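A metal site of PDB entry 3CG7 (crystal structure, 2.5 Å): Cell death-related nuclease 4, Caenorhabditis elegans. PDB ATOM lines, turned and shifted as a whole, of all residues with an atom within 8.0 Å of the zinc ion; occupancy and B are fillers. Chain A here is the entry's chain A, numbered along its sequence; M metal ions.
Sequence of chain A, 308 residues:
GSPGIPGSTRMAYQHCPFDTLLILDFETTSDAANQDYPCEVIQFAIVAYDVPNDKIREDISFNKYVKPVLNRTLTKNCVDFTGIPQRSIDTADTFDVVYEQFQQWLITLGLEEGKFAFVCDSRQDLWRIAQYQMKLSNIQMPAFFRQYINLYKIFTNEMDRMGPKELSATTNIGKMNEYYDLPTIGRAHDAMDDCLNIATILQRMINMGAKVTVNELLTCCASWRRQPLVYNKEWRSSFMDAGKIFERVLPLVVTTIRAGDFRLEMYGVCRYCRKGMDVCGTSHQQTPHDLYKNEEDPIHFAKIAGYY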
ATOM      1  N   ARG A 146     -14.097   5.756   5.900  1.00  0.00           N
ATOM      2  CA  ARG A 146     -12.677   5.721   6.282  1.00  0.00           C
ATOM      3  C   ARG A 146     -11.719   5.518   5.088  1.00  0.00           C
ATOM      4  O   ARG A 146     -10.497   5.448   5.257  1.00  0.00           O
ATOM      5  CB  ARG A 146     -12.434   4.710   7.403  1.00  0.00           C
ATOM      6  CG  ARG A 146     -13.091   5.123   8.724  1.00  0.00           C
ATOM      7  CD  ARG A 146     -12.675   4.233   9.882  1.00  0.00           C
ATOM      8  NE  ARG A 146     -11.227   4.215  10.054  1.00  0.00           N
ATOM      9  CZ  ARG A 146     -10.588   3.593  11.037  1.00  0.00           C
ATOM     10  NH1 ARG A 146     -11.272   2.926  11.975  1.00  0.00           N
ATOM     11  NH2 ARG A 146      -9.260   3.637  11.089  1.00  0.00           N
ATOM     12  N   LEU A 218      -8.464   7.076   6.463  1.00  0.00           N
ATOM     13  CA  LEU A 218      -8.494   7.555   7.838  1.00  0.00           C
ATOM     14  C   LEU A 218      -7.932   6.494   8.759  1.00  0.00           C
ATOM     15  O   LEU A 218      -8.414   5.366   8.811  1.00  0.00           O
ATOM     16  CB  LEU A 218      -9.904   7.966   8.262  1.00  0.00           C
ATOM     17  CG  LEU A 218     -10.503   9.124   7.454  1.00  0.00           C
ATOM     18  CD1 LEU A 218     -11.914   9.403   7.917  1.00  0.00           C
ATOM     19  CD2 LEU A 218      -9.630  10.361   7.568  1.00  0.00           C
ATOM     20  N   THR A 219      -6.889   6.884   9.490  1.00  0.00           N
ATOM     21  CA  THR A 219      -6.136   5.959  10.301  1.00  0.00           C
ATOM     22  C   THR A 219      -6.094   6.436  11.759  1.00  0.00           C
ATOM     23  O   THR A 219      -6.260   7.626  12.032  1.00  0.00           O
ATOM     24  CB  THR A 219      -4.724   5.753   9.706  1.00  0.00           C
ATOM     25  OG1 THR A 219      -4.166   4.524  10.204  1.00  0.00           O
ATOM     26  CG2 THR A 219      -3.788   6.904  10.055  1.00  0.00           C
ATOM     27  N   CYS A 220      -5.881   5.510  12.681  1.00  0.00           N
ATOM     28  CA  CYS A 220      -5.921   5.827  14.114  1.00  0.00           C
ATOM     29  C   CYS A 220      -4.624   6.437  14.642  1.00  0.00           C
ATOM     30  O   CYS A 220      -4.588   6.934  15.773  1.00  0.00           O
ATOM     31  CB  CYS A 220      -6.264   4.588  14.917  1.00  0.00           C
ATOM     32  SG  CYS A 220      -5.073   3.248  14.704  1.00  0.00           S
ATOM     33  N   CYS A 221      -3.562   6.403  13.850  1.00  0.00           N
ATOM     34  CA  CYS A 221      -2.247   6.784  14.358  1.00  0.00           C
ATOM     35  C   CYS A 221      -1.323   7.416  13.329  1.00  0.00           C
ATOM     36  O   CYS A 221      -1.294   7.010  12.170  1.00  0.00           O
ATOM     37  CB  CYS A 221      -1.585   5.572  14.991  1.00  0.00           C
ATOM     38  SG  CYS A 221      -0.258   5.984  16.111  1.00  0.00           S
ATOM     39  N   LEU A 252      -9.115   9.923  14.412  1.00  0.00           N
ATOM     40  CA  LEU A 252      -8.643   9.447  13.105  1.00  0.00           C
ATOM     41  C   LEU A 252      -7.979  10.530  12.284  1.00  0.00           C
ATOM     42  O   LEU A 252      -8.427  11.666  12.259  1.00  0.00           O
ATOM     43  CB  LEU A 252      -9.764   8.787  12.304  1.00  0.00           C
ATOM     44  CG  LEU A 252     -10.540   7.667  13.009  1.00  0.00           C
ATOM     45  CD1 LEU A 252     -11.655   7.130  12.113  1.00  0.00           C
ATOM     46  CD2 LEU A 252      -9.620   6.533  13.486  1.00  0.00           C
ATOM     47  N   VAL A 269     -10.138  -2.327   6.766  1.00  0.00           N
ATOM     48  CA  VAL A 269      -9.107  -2.585   7.760  1.00  0.00           C
ATOM     49  C   VAL A 269      -8.211  -1.347   7.853  1.00  0.00           C
ATOM     50  O   VAL A 269      -7.919  -0.693   6.844  1.00  0.00           O
ATOM     51  CB  VAL A 269      -8.264  -3.896   7.452  1.00  0.00           C
ATOM     52  CG1 VAL A 269      -9.151  -4.988   6.810  1.00  0.00           C
ATOM     53  CG2 VAL A 269      -7.042  -3.616   6.568  1.00  0.00           C
ATOM     54  N   CYS A 270      -7.803  -1.018   9.069  1.00  0.00           N
ATOM     55  CA  CYS A 270      -7.009   0.175   9.304  1.00  0.00           C
ATOM     56  C   CYS A 270      -5.582  -0.013   8.788  1.00  0.00           C
ATOM     57  O   CYS A 270      -4.966  -1.044   9.041  1.00  0.00           O
ATOM     58  CB  CYS A 270      -7.018   0.521  10.789  1.00  0.00           C
ATOM     59  SG  CYS A 270      -6.048   1.970  11.206  1.00  0.00           S
ATOM     60  N   ARG A 271      -5.072   0.975   8.060  1.00  0.00           N
ATOM     61  CA  ARG A 271      -3.724   0.899   7.457  1.00  0.00           C
ATOM     62  C   ARG A 271      -2.626   0.761   8.487  1.00  0.00           C
ATOM     63  O   ARG A 271      -1.579   0.162   8.202  1.00  0.00           O
ATOM     64  CB  ARG A 271      -3.432   2.110   6.564  1.00  0.00           C
ATOM     65  CG  ARG A 271      -4.319   2.226   5.350  1.00  0.00           C
ATOM     66  CD  ARG A 271      -3.793   1.438   4.136  1.00  0.00           C
ATOM     67  NE  ARG A 271      -3.772  -0.018   4.326  1.00  0.00           N
ATOM     68  CZ  ARG A 271      -4.846  -0.786   4.490  1.00  0.00           C
ATOM     69  NH1 ARG A 271      -6.065  -0.251   4.513  1.00  0.00           N
ATOM     70  NH2 ARG A 271      -4.696  -2.090   4.652  1.00  0.00           N
ATOM     71  N   TYR A 272      -2.843   1.304   9.680  1.00  0.00           N
ATOM     72  CA  TYR A 272      -1.840   1.244  10.741  1.00  0.00           C
ATOM     73  C   TYR A 272      -1.974   0.005  11.616  1.00  0.00           C
ATOM     74  O   TYR A 272      -1.055  -0.816  11.662  1.00  0.00           O
ATOM     75  CB  TYR A 272      -1.848   2.519  11.596  1.00  0.00           C
ATOM     76  CG  TYR A 272      -0.828   2.497  12.709  1.00  0.00           C
ATOM     77  CD1 TYR A 272       0.504   2.830  12.472  1.00  0.00           C
ATOM     78  CD2 TYR A 272      -1.200   2.144  14.019  1.00  0.00           C
ATOM     79  CE1 TYR A 272       1.445   2.810  13.509  1.00  0.00           C
ATOM     80  CE2 TYR A 272      -0.273   2.124  15.055  1.00  0.00           C
ATOM     81  CZ  TYR A 272       1.046   2.457  14.789  1.00  0.00           C
ATOM     82  OH  TYR A 272       1.967   2.437  15.818  1.00  0.00           O
ATOM     83  N   CYS A 273      -3.098  -0.149  12.298  1.00  0.00           N
ATOM     84  CA  CYS A 273      -3.251  -1.211  13.297  1.00  0.00           C
ATOM     85  C   CYS A 273      -3.713  -2.539  12.692  1.00  0.00           C
ATOM     86  O   CYS A 273      -3.730  -3.570  13.376  1.00  0.00           O
ATOM     87  CB  CYS A 273      -4.165  -0.776  14.445  1.00  0.00           C
ATOM     88  SG  CYS A 273      -5.916  -0.653  14.021  1.00  0.00           S
ATOM     89  N   ARG A 274      -4.091  -2.505  11.419  1.00  0.00           N
ATOM     90  CA  ARG A 274      -4.457  -3.697  10.640  1.00  0.00           C
ATOM     91  C   ARG A 274      -5.659  -4.458  11.206  1.00  0.00           C
ATOM     92  O   ARG A 274      -5.893  -5.621  10.856  1.00  0.00           O
ATOM     93  CB  ARG A 274      -3.237  -4.617  10.449  1.00  0.00           C
ATOM     94  CG  ARG A 274      -2.033  -3.932   9.775  1.00  0.00           C
ATOM     95  CD  ARG A 274      -2.167  -3.918   8.248  1.00  0.00           C
ATOM     96  NE  ARG A 274      -1.504  -2.762   7.642  1.00  0.00           N
ATOM     97  CZ  ARG A 274      -1.068  -2.719   6.376  1.00  0.00           C
ATOM     98  NH1 ARG A 274      -1.200  -3.767   5.569  1.00  0.00           N
ATOM     99  NH2 ARG A 274      -0.487  -1.608   5.919  1.00  0.00           N
ATOM    100  N   LYS A 275      -6.429  -3.793  12.073  1.00  0.00           N
ATOM    101  CA  LYS A 275      -7.634  -4.385  12.658  1.00  0.00           C
ATOM    102  C   LYS A 275      -8.894  -3.879  11.961  1.00  0.00           C
ATOM    103  O   LYS A 275      -8.891  -2.800  11.371  1.00  0.00           O
ATOM    104  CB  LYS A 275      -7.728  -4.040  14.152  1.00  0.00           C
ATOM    105  CG  LYS A 275      -6.565  -4.523  15.013  1.00  0.00           C
ATOM    106  CD  LYS A 275      -6.698  -3.966  16.425  1.00  0.00           C
ATOM    107  CE  LYS A 275      -5.361  -3.983  17.170  1.00  0.00           C
ATOM    108  NZ  LYS A 275      -5.489  -3.324  18.501  1.00  0.00           N
ATOM    109  N   GLY A 276      -9.962  -4.674  12.039  1.00  0.00           N
ATOM    110  CA  GLY A 276     -11.258  -4.302  11.463  1.00  0.00           C
ATOM    111  C   GLY A 276     -11.691  -2.942  11.986  1.00  0.00           C
ATOM    112  O   GLY A 276     -11.311  -2.530  13.081  1.00  0.00           O
ATOM    113  N   MET A 277     -12.507  -2.238  11.198  1.00  0.00           N
ATOM    114  CA  MET A 277     -12.922  -0.893  11.572  1.00  0.00           C
ATOM    115  C   MET A 277     -14.077  -0.866  12.563  1.00  0.00           C
ATOM    116  O   MET A 277     -14.568   0.207  12.944  1.00  0.00           O
ATOM    117  CB  MET A 277     -13.154  -0.028  10.320  1.00  0.00           C
ATOM    118  CG  MET A 277     -11.834   0.456   9.725  1.00  0.00           C
ATOM    119  SD  MET A 277     -11.959   0.966   8.016  1.00  0.00           S
ATOM    120  CE  MET A 277     -10.313   1.625   7.698  1.00  0.00           C
ATOM    121  N   VAL A 279     -13.419  -2.455  15.418  1.00  0.00           N
ATOM    122  CA  VAL A 279     -12.582  -2.451  16.626  1.00  0.00           C
ATOM    123  C   VAL A 279     -11.721  -1.182  16.697  1.00  0.00           C
ATOM    124  O   VAL A 279     -11.596  -0.572  17.767  1.00  0.00           O
ATOM    125  CB  VAL A 279     -11.682  -3.723  16.692  1.00  0.00           C
ATOM    126  CG1 VAL A 279     -10.813  -3.730  17.952  1.00  0.00           C
ATOM    127  CG2 VAL A 279     -12.515  -5.001  16.623  1.00  0.00           C
ATOM    128  N   CYS A 280     -11.127  -0.781  15.566  1.00  0.00           N
ATOM    129  CA  CYS A 280     -10.328   0.440  15.518  1.00  0.00           C
ATOM    130  C   CYS A 280     -11.233   1.663  15.428  1.00  0.00           C
ATOM    131  O   CYS A 280     -12.208   1.674  14.672  1.00  0.00           O
ATOM    132  CB  CYS A 280      -9.364   0.407  14.322  1.00  0.00           C
ATOM    133  SG  CYS A 280      -8.542   1.997  14.011  1.00  0.00           S
ATOM    134  N   GLY A 281     -10.886   2.695  16.194  1.00  0.00           N
ATOM    135  CA  GLY A 281     -11.605   3.948  16.168  1.00  0.00           C
ATOM    136  C   GLY A 281     -12.562   4.172  17.334  1.00  0.00           C
ATOM    137  O   GLY A 281     -13.242   5.193  17.389  1.00  0.00           O
ATOM    138  N   THR A 282     -12.617   3.213  18.251  1.00  0.00           N
ATOM    139  CA  THR A 282     -13.461   3.358  19.437  1.00  0.00           C
ATOM    140  C   THR A 282     -12.803   4.286  20.448  1.00  0.00           C
ATOM    141  O   THR A 282     -13.477   4.904  21.271  1.00  0.00           O
ATOM    142  CB  THR A 282     -13.759   2.003  20.134  1.00  0.00           C
ATOM    143  OG1 THR A 282     -13.605   0.922  19.211  1.00  0.00           O
ATOM    144  CG2 THR A 282     -15.187   1.989  20.686  1.00  0.00           C
ATOM    145  N   SER A 283     -11.473   4.394  20.368  1.00  0.00           N
ATOM    146  CA  SER A 283     -10.708   5.103  21.386  1.00  0.00           C
ATOM    147  C   SER A 283      -9.510   5.825  20.783  1.00  0.00           C
ATOM    148  O   SER A 283      -8.671   5.205  20.121  1.00  0.00           O
ATOM    149  CB  SER A 283     -10.257   4.106  22.458  1.00  0.00           C
ATOM    150  OG  SER A 283      -9.901   4.754  23.659  1.00  0.00           O
ATOM    151  N   GLN A 285      -6.002   7.117  20.119  1.00  0.00           N
ATOM    152  CA  GLN A 285      -4.748   6.433  20.420  1.00  0.00           C
ATOM    153  C   GLN A 285      -3.605   7.419  20.665  1.00  0.00           C
ATOM    154  O   GLN A 285      -2.502   7.020  21.063  1.00  0.00           O
ATOM    155  CB  GLN A 285      -4.354   5.471  19.290  1.00  0.00           C
ATOM    156  CG  GLN A 285      -5.379   4.357  18.993  1.00  0.00           C
ATOM    157  CD  GLN A 285      -5.520   3.341  20.129  1.00  0.00           C
ATOM    158  OE1 GLN A 285      -6.625   3.044  20.567  1.00  0.00           O
ATOM    159  NE2 GLN A 285      -4.391   2.810  20.582  1.00  0.00           N
HETATM  160 ZN    ZN M   1      -6.392   1.574  13.631  1.00  0.00          ZN
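O of Lys 275 is in hydrogen-bond range of N of Cys 270 (3.1 Å).
The side-chain sulfur (SG) of Cys 270 lies close to the guanidinium group (NH2) of Arg 146 (3.6 Å).
The side-chain sulfur (SG) of Cys 270 lies close to the backbone NH (N) of Tyr 272 (3.6 Å).
O of Cys 280 is in hydrogen-bond range of NH1 of Arg 146, 3.1 Å away.
The backbone NH (N) of Lys 275 sits close to the side-chain sulfur (SG) of Cys 273.
The side-chain sulfur (SG) of Cys 270 sits close to the side-chain hydroxyl (OG1) of Thr 219, 3.3 Å away.
Four residues have an atom within 4 Å of the zinc ion: Cys 220, Cys 270, Cys 273 and Cys 280.
The zinc ion is bound by the side-chain sulfur (SG) of Cys 280 (2.2 Å).
The zinc ion is bound by SG of Cys 273, at 2.3 Å.
The zinc ion is bound by SG of Cys 220 (2.4 Å).
The side-chain sulfur (SG) of Cys 270 is bound to the zinc ion, 2.5 Å away.
The zinc ion has four donor atoms within binding distance.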
